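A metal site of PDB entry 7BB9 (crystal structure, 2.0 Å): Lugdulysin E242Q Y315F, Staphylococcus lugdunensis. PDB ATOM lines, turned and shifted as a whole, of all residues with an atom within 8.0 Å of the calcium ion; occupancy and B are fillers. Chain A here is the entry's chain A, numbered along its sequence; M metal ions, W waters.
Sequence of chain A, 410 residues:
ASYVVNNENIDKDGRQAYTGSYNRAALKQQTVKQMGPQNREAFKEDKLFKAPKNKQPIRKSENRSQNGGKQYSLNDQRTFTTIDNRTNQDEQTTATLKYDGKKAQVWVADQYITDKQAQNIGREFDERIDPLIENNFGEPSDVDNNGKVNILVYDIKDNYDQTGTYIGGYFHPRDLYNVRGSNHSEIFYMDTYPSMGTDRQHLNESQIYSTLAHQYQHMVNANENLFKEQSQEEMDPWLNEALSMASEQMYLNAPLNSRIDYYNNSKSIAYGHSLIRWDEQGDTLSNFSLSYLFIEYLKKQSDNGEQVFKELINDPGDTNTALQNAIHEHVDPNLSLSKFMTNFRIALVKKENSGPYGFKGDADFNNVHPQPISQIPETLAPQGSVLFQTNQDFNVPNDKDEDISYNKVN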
ATOM      1  N   ASN A  85      10.526  20.650  33.064  1.00  0.00           N
ATOM      2  CA  ASN A  85      10.686  22.071  32.802  1.00  0.00           C
ATOM      3  C   ASN A  85       9.717  22.928  33.593  1.00  0.00           C
ATOM      4  O   ASN A  85       9.813  24.151  33.541  1.00  0.00           O
ATOM      5  CB  ASN A  85      10.519  22.368  31.320  1.00  0.00           C
ATOM      6  CG  ASN A  85      11.560  21.651  30.483  1.00  0.00           C
ATOM      7  OD1 ASN A  85      12.703  22.080  30.396  1.00  0.00           O
ATOM      8  ND2 ASN A  85      11.170  20.528  29.920  1.00  0.00           N
ATOM      9  N   ASP A 110       5.900   7.066  26.719  1.00  0.00           N
ATOM     10  CA  ASP A 110       4.514   7.513  26.873  1.00  0.00           C
ATOM     11  C   ASP A 110       3.618   6.349  26.486  1.00  0.00           C
ATOM     12  O   ASP A 110       3.617   5.921  25.323  1.00  0.00           O
ATOM     13  CB  ASP A 110       4.230   8.740  25.999  1.00  0.00           C
ATOM     14  CG  ASP A 110       2.813   9.293  26.188  1.00  0.00           C
ATOM     15  OD1 ASP A 110       1.914   8.505  26.548  1.00  0.00           O
ATOM     16  OD2 ASP A 110       2.605  10.506  25.996  1.00  0.00           O
ATOM     17  N   TYR A 154       8.383  11.049  24.612  1.00  0.00           N
ATOM     18  CA  TYR A 154       7.672  10.968  25.878  1.00  0.00           C
ATOM     19  C   TYR A 154       6.995  12.298  26.133  1.00  0.00           C
ATOM     20  O   TYR A 154       7.201  13.276  25.395  1.00  0.00           O
ATOM     21  CB  TYR A 154       8.626  10.613  27.046  1.00  0.00           C
ATOM     22  CG  TYR A 154       9.377  11.795  27.644  1.00  0.00           C
ATOM     23  CD1 TYR A 154      10.490  12.342  27.006  1.00  0.00           C
ATOM     24  CD2 TYR A 154       8.985  12.353  28.857  1.00  0.00           C
ATOM     25  CE1 TYR A 154      11.187  13.433  27.567  1.00  0.00           C
ATOM     26  CE2 TYR A 154       9.653  13.435  29.411  1.00  0.00           C
ATOM     27  CZ  TYR A 154      10.742  13.968  28.760  1.00  0.00           C
ATOM     28  OH  TYR A 154      11.398  15.035  29.329  1.00  0.00           O
ATOM     29  N   ASP A 155       6.194  12.356  27.203  1.00  0.00           N
ATOM     30  CA  ASP A 155       5.472  13.580  27.557  1.00  0.00           C
ATOM     31  C   ASP A 155       6.401  14.477  28.353  1.00  0.00           C
ATOM     32  O   ASP A 155       6.539  14.330  29.566  1.00  0.00           O
ATOM     33  CB  ASP A 155       4.211  13.269  28.367  1.00  0.00           C
ATOM     34  CG  ASP A 155       3.367  14.518  28.658  1.00  0.00           C
ATOM     35  OD1 ASP A 155       3.732  15.621  28.214  1.00  0.00           O
ATOM     36  OD2 ASP A 155       2.330  14.386  29.339  1.00  0.00           O
ATOM     37  N   ILE A 156       7.013  15.442  27.668  1.00  0.00           N
ATOM     38  CA  ILE A 156       7.848  16.411  28.346  1.00  0.00           C
ATOM     39  C   ILE A 156       7.000  17.237  29.300  1.00  0.00           C
ATOM     40  O   ILE A 156       5.930  17.737  28.934  1.00  0.00           O
ATOM     41  CB  ILE A 156       8.549  17.307  27.306  1.00  0.00           C
ATOM     42  CG1 ILE A 156       9.406  16.437  26.361  1.00  0.00           C
ATOM     43  CG2 ILE A 156       9.346  18.386  28.025  1.00  0.00           C
ATOM     44  CD1 ILE A 156      10.094  17.216  25.217  1.00  0.00           C
ATOM     45  N   LYS A 157       7.482  17.384  30.533  1.00  0.00           N
ATOM     46  CA  LYS A 157       6.766  18.133  31.564  1.00  0.00           C
ATOM     47  C   LYS A 157       7.089  19.606  31.464  1.00  0.00           C
ATOM     48  O   LYS A 157       8.260  19.993  31.372  1.00  0.00           O
ATOM     49  CB  LYS A 157       7.129  17.614  32.961  1.00  0.00           C
ATOM     50  CG  LYS A 157       6.548  16.267  33.334  1.00  0.00           C
ATOM     51  CD  LYS A 157       6.743  16.011  34.814  1.00  0.00           C
ATOM     52  CE  LYS A 157       6.401  14.575  35.206  1.00  0.00           C
ATOM     53  NZ  LYS A 157       6.049  14.480  36.654  1.00  0.00           N
ATOM     54  N   ASP A 158       6.054  20.440  31.528  1.00  0.00           N
ATOM     55  CA  ASP A 158       6.179  21.883  31.328  1.00  0.00           C
ATOM     56  C   ASP A 158       4.956  22.545  31.972  1.00  0.00           C
ATOM     57  O   ASP A 158       4.208  21.912  32.724  1.00  0.00           O
ATOM     58  CB  ASP A 158       6.325  22.225  29.841  1.00  0.00           C
ATOM     59  CG  ASP A 158       5.139  21.759  28.996  1.00  0.00           C
ATOM     60  OD1 ASP A 158       4.104  21.372  29.579  1.00  0.00           O
ATOM     61  OD2 ASP A 158       5.217  21.778  27.743  1.00  0.00           O
ATOM     62  N   ASN A 159       4.731  23.819  31.653  1.00  0.00           N
ATOM     63  CA  ASN A 159       3.606  24.585  32.175  1.00  0.00           C
ATOM     64  C   ASN A 159       2.467  24.727  31.169  1.00  0.00           C
ATOM     65  O   ASN A 159       1.670  25.662  31.257  1.00  0.00           O
ATOM     66  CB  ASN A 159       4.086  25.973  32.618  1.00  0.00           C
ATOM     67  CG  ASN A 159       4.889  25.917  33.893  1.00  0.00           C
ATOM     68  OD1 ASN A 159       6.068  26.305  33.923  1.00  0.00           O
ATOM     69  ND2 ASN A 159       4.268  25.416  34.966  1.00  0.00           N
ATOM     70  N   TYR A 160       2.366  23.807  30.203  1.00  0.00           N
ATOM     71  CA  TYR A 160       1.341  23.918  29.191  1.00  0.00           C
ATOM     72  C   TYR A 160      -0.054  24.001  29.815  1.00  0.00           C
ATOM     73  O   TYR A 160      -0.834  24.904  29.494  1.00  0.00           O
ATOM     74  CB  TYR A 160       1.424  22.746  28.214  1.00  0.00           C
ATOM     75  CG  TYR A 160       0.272  22.733  27.260  1.00  0.00           C
ATOM     76  CD1 TYR A 160       0.155  23.712  26.289  1.00  0.00           C
ATOM     77  CD2 TYR A 160      -0.730  21.771  27.369  1.00  0.00           C
ATOM     78  CE1 TYR A 160      -0.914  23.717  25.422  1.00  0.00           C
ATOM     79  CE2 TYR A 160      -1.798  21.761  26.515  1.00  0.00           C
ATOM     80  CZ  TYR A 160      -1.893  22.744  25.547  1.00  0.00           C
ATOM     81  OH  TYR A 160      -2.968  22.730  24.688  1.00  0.00           O
ATOM     82  N   ASP A 161      -0.360  23.074  30.720  1.00  0.00           N
ATOM     83  CA  ASP A 161      -1.673  23.008  31.360  1.00  0.00           C
ATOM     84  C   ASP A 161      -2.089  24.337  31.979  1.00  0.00           C
ATOM     85  O   ASP A 161      -3.284  24.593  32.116  1.00  0.00           O
ATOM     86  CB  ASP A 161      -1.677  21.928  32.445  1.00  0.00           C
ATOM     87  CG  ASP A 161      -1.618  20.520  31.874  1.00  0.00           C
ATOM     88  OD1 ASP A 161      -1.945  20.341  30.677  1.00  0.00           O
ATOM     89  OD2 ASP A 161      -1.222  19.603  32.633  1.00  0.00           O
ATOM     90  N   TYR A 166       3.921  25.331  25.308  1.00  0.00           N
ATOM     91  CA  TYR A 166       4.376  23.969  25.524  1.00  0.00           C
ATOM     92  C   TYR A 166       5.751  23.777  24.912  1.00  0.00           C
ATOM     93  O   TYR A 166       6.160  24.518  24.025  1.00  0.00           O
ATOM     94  CB  TYR A 166       3.413  22.918  24.952  1.00  0.00           C
ATOM     95  CG  TYR A 166       3.251  22.953  23.443  1.00  0.00           C
ATOM     96  CD1 TYR A 166       2.319  23.802  22.832  1.00  0.00           C
ATOM     97  CD2 TYR A 166       4.015  22.130  22.611  1.00  0.00           C
ATOM     98  CE1 TYR A 166       2.145  23.817  21.454  1.00  0.00           C
ATOM     99  CE2 TYR A 166       3.856  22.138  21.239  1.00  0.00           C
ATOM    100  CZ  TYR A 166       2.922  22.978  20.664  1.00  0.00           C
ATOM    101  OH  TYR A 166       2.785  22.983  19.300  1.00  0.00           O
ATOM    102  N   ILE A 167       6.438  22.747  25.393  1.00  0.00           N
ATOM    103  CA  ILE A 167       7.804  22.471  24.978  1.00  0.00           C
ATOM    104  C   ILE A 167       7.752  21.253  24.058  1.00  0.00           C
ATOM    105  O   ILE A 167       7.237  20.191  24.447  1.00  0.00           O
ATOM    106  CB  ILE A 167       8.713  22.272  26.195  1.00  0.00           C
ATOM    107  CG1 ILE A 167       9.102  23.641  26.752  1.00  0.00           C
ATOM    108  CG2 ILE A 167       9.973  21.482  25.828  1.00  0.00           C
ATOM    109  CD1 ILE A 167       9.491  23.639  28.193  1.00  0.00           C
ATOM    110  N   GLY A 168       8.239  21.433  22.830  1.00  0.00           N
ATOM    111  CA  GLY A 168       8.130  20.409  21.805  1.00  0.00           C
ATOM    112  C   GLY A 168       9.292  19.430  21.832  1.00  0.00           C
ATOM    113  O   GLY A 168       9.166  18.308  21.328  1.00  0.00           O
ATOM    114  N   MET A 190      11.823  14.408  22.496  1.00  0.00           N
ATOM    115  CA  MET A 190      10.699  14.800  21.656  1.00  0.00           C
ATOM    116  C   MET A 190       9.404  14.634  22.439  1.00  0.00           C
ATOM    117  O   MET A 190       9.164  13.575  23.026  1.00  0.00           O
ATOM    118  CB  MET A 190      10.641  13.950  20.379  1.00  0.00           C
ATOM    119  CG  MET A 190      11.792  14.209  19.430  1.00  0.00           C
ATOM    120  SD  MET A 190      11.611  15.906  18.859  1.00  0.00           S
ATOM    121  CE  MET A 190      13.056  16.126  17.917  1.00  0.00           C
ATOM    122  N   ASP A 191       8.571  15.660  22.423  1.00  0.00           N
ATOM    123  CA  ASP A 191       7.357  15.665  23.225  1.00  0.00           C
ATOM    124  C   ASP A 191       6.200  15.004  22.488  1.00  0.00           C
ATOM    125  O   ASP A 191       6.080  15.096  21.254  1.00  0.00           O
ATOM    126  CB  ASP A 191       6.961  17.098  23.561  1.00  0.00           C
ATOM    127  CG  ASP A 191       5.685  17.165  24.383  1.00  0.00           C
ATOM    128  OD1 ASP A 191       5.710  16.678  25.539  1.00  0.00           O
ATOM    129  OD2 ASP A 191       4.681  17.694  23.871  1.00  0.00           O
ATOM    130  N   THR A 192       5.318  14.366  23.251  1.00  0.00           N
ATOM    131  CA  THR A 192       4.120  13.742  22.686  1.00  0.00           C
ATOM    132  C   THR A 192       2.913  14.674  22.810  1.00  0.00           C
ATOM    133  O   THR A 192       2.444  15.213  21.806  1.00  0.00           O
ATOM    134  CB  THR A 192       3.857  12.400  23.362  1.00  0.00           C
ATOM    135  OG1 THR A 192       3.908  12.560  24.791  1.00  0.00           O
ATOM    136  CG2 THR A 192       4.949  11.420  22.966  1.00  0.00           C
ATOM    137  N   TYR A 193       2.416  14.882  24.030  1.00  0.00           N
ATOM    138  CA  TYR A 193       1.269  15.738  24.335  1.00  0.00           C
ATOM    139  C   TYR A 193       1.736  17.064  24.939  1.00  0.00           C
ATOM    140  O   TYR A 193       2.434  17.048  25.967  1.00  0.00           O
ATOM    141  CB  TYR A 193       0.314  15.036  25.296  1.00  0.00           C
ATOM    142  CG  TYR A 193      -0.759  15.933  25.839  1.00  0.00           C
ATOM    143  CD1 TYR A 193      -1.931  16.160  25.122  1.00  0.00           C
ATOM    144  CD2 TYR A 193      -0.602  16.587  27.059  1.00  0.00           C
ATOM    145  CE1 TYR A 193      -2.920  16.998  25.601  1.00  0.00           C
ATOM    146  CE2 TYR A 193      -1.590  17.442  27.542  1.00  0.00           C
ATOM    147  CZ  TYR A 193      -2.742  17.631  26.808  1.00  0.00           C
ATOM    148  OH  TYR A 193      -3.723  18.474  27.292  1.00  0.00           O
ATOM    149  N   PRO A 194       1.331  18.226  24.391  1.00  0.00           N
ATOM    150  CA  PRO A 194       0.372  18.341  23.282  1.00  0.00           C
ATOM    151  C   PRO A 194       0.992  18.638  21.925  1.00  0.00           C
ATOM    152  O   PRO A 194       0.261  19.107  21.044  1.00  0.00           O
ATOM    153  CB  PRO A 194      -0.487  19.518  23.723  1.00  0.00           C
ATOM    154  CG  PRO A 194       0.571  20.462  24.310  1.00  0.00           C
ATOM    155  CD  PRO A 194       1.631  19.543  24.976  1.00  0.00           C
ATOM    156  N   SER A 195       2.306  18.402  21.765  1.00  0.00           N
ATOM    157  CA  SER A 195       2.972  18.696  20.491  1.00  0.00           C
ATOM    158  C   SER A 195       2.324  17.933  19.335  1.00  0.00           C
ATOM    159  O   SER A 195       2.143  18.485  18.244  1.00  0.00           O
ATOM    160  CB  SER A 195       4.458  18.345  20.559  1.00  0.00           C
ATOM    161  OG  SER A 195       5.123  19.090  21.568  1.00  0.00           O
ATOM    162  N   ARG A 200      -4.854  13.100  23.848  1.00  0.00           N
ATOM    163  CA  ARG A 200      -3.836  12.091  24.136  1.00  0.00           C
ATOM    164  C   ARG A 200      -4.092  10.780  23.398  1.00  0.00           C
ATOM    165  O   ARG A 200      -3.140  10.040  23.131  1.00  0.00           O
ATOM    166  CB  ARG A 200      -3.765  11.803  25.642  1.00  0.00           C
ATOM    167  CG  ARG A 200      -3.438  13.026  26.484  1.00  0.00           C
ATOM    168  CD  ARG A 200      -3.098  12.675  27.925  1.00  0.00           C
ATOM    169  NE  ARG A 200      -1.681  12.921  28.189  1.00  0.00           N
ATOM    170  CZ  ARG A 200      -1.215  13.864  28.994  1.00  0.00           C
ATOM    171  NH1 ARG A 200      -2.038  14.673  29.648  1.00  0.00           N
ATOM    172  NH2 ARG A 200       0.088  13.998  29.144  1.00  0.00           N
HETATM  173 CA    CA M   1       4.350  17.627  27.215  1.00  0.00          CA
HETATM  174  O   HOH W   1       5.148  19.665  26.183  1.00  0.00           O
HETATM  175  O   HOH W   2       2.916  19.232  28.618  1.00  0.00           O
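The calcium ion is bound by the side-chain carboxylate (OD1) of Asp 155 (2.3 Å), the backbone carbonyl oxygen (O) of Ile 156 (2.3 Å), the side-chain carboxylate (OD1) of Asp 191 (2.4 Å), the backbone carbonyl oxygen (O) of Tyr 193 (2.4 Å), water W1 (2.4 Å) and water W2 (2.6 Å).
The backbone NH (N) of Asp 155 is in hydrogen-bond range of the side-chain hydroxyl (OG1) of Thr 192 (3.3 Å). OD2 of Asp 191 lies within hydrogen-bond range of OG of Ser 195. O of Gly 168 lies within hydrogen-bond range of N of Asp 191.
Four residues have an atom within 4 Å of the calcium ion: Asp 155, Ile 156, Asp 191 and Tyr 193. The nearest printed residue that does not touch the calcium ion is Pro 194 (4.01 Å).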
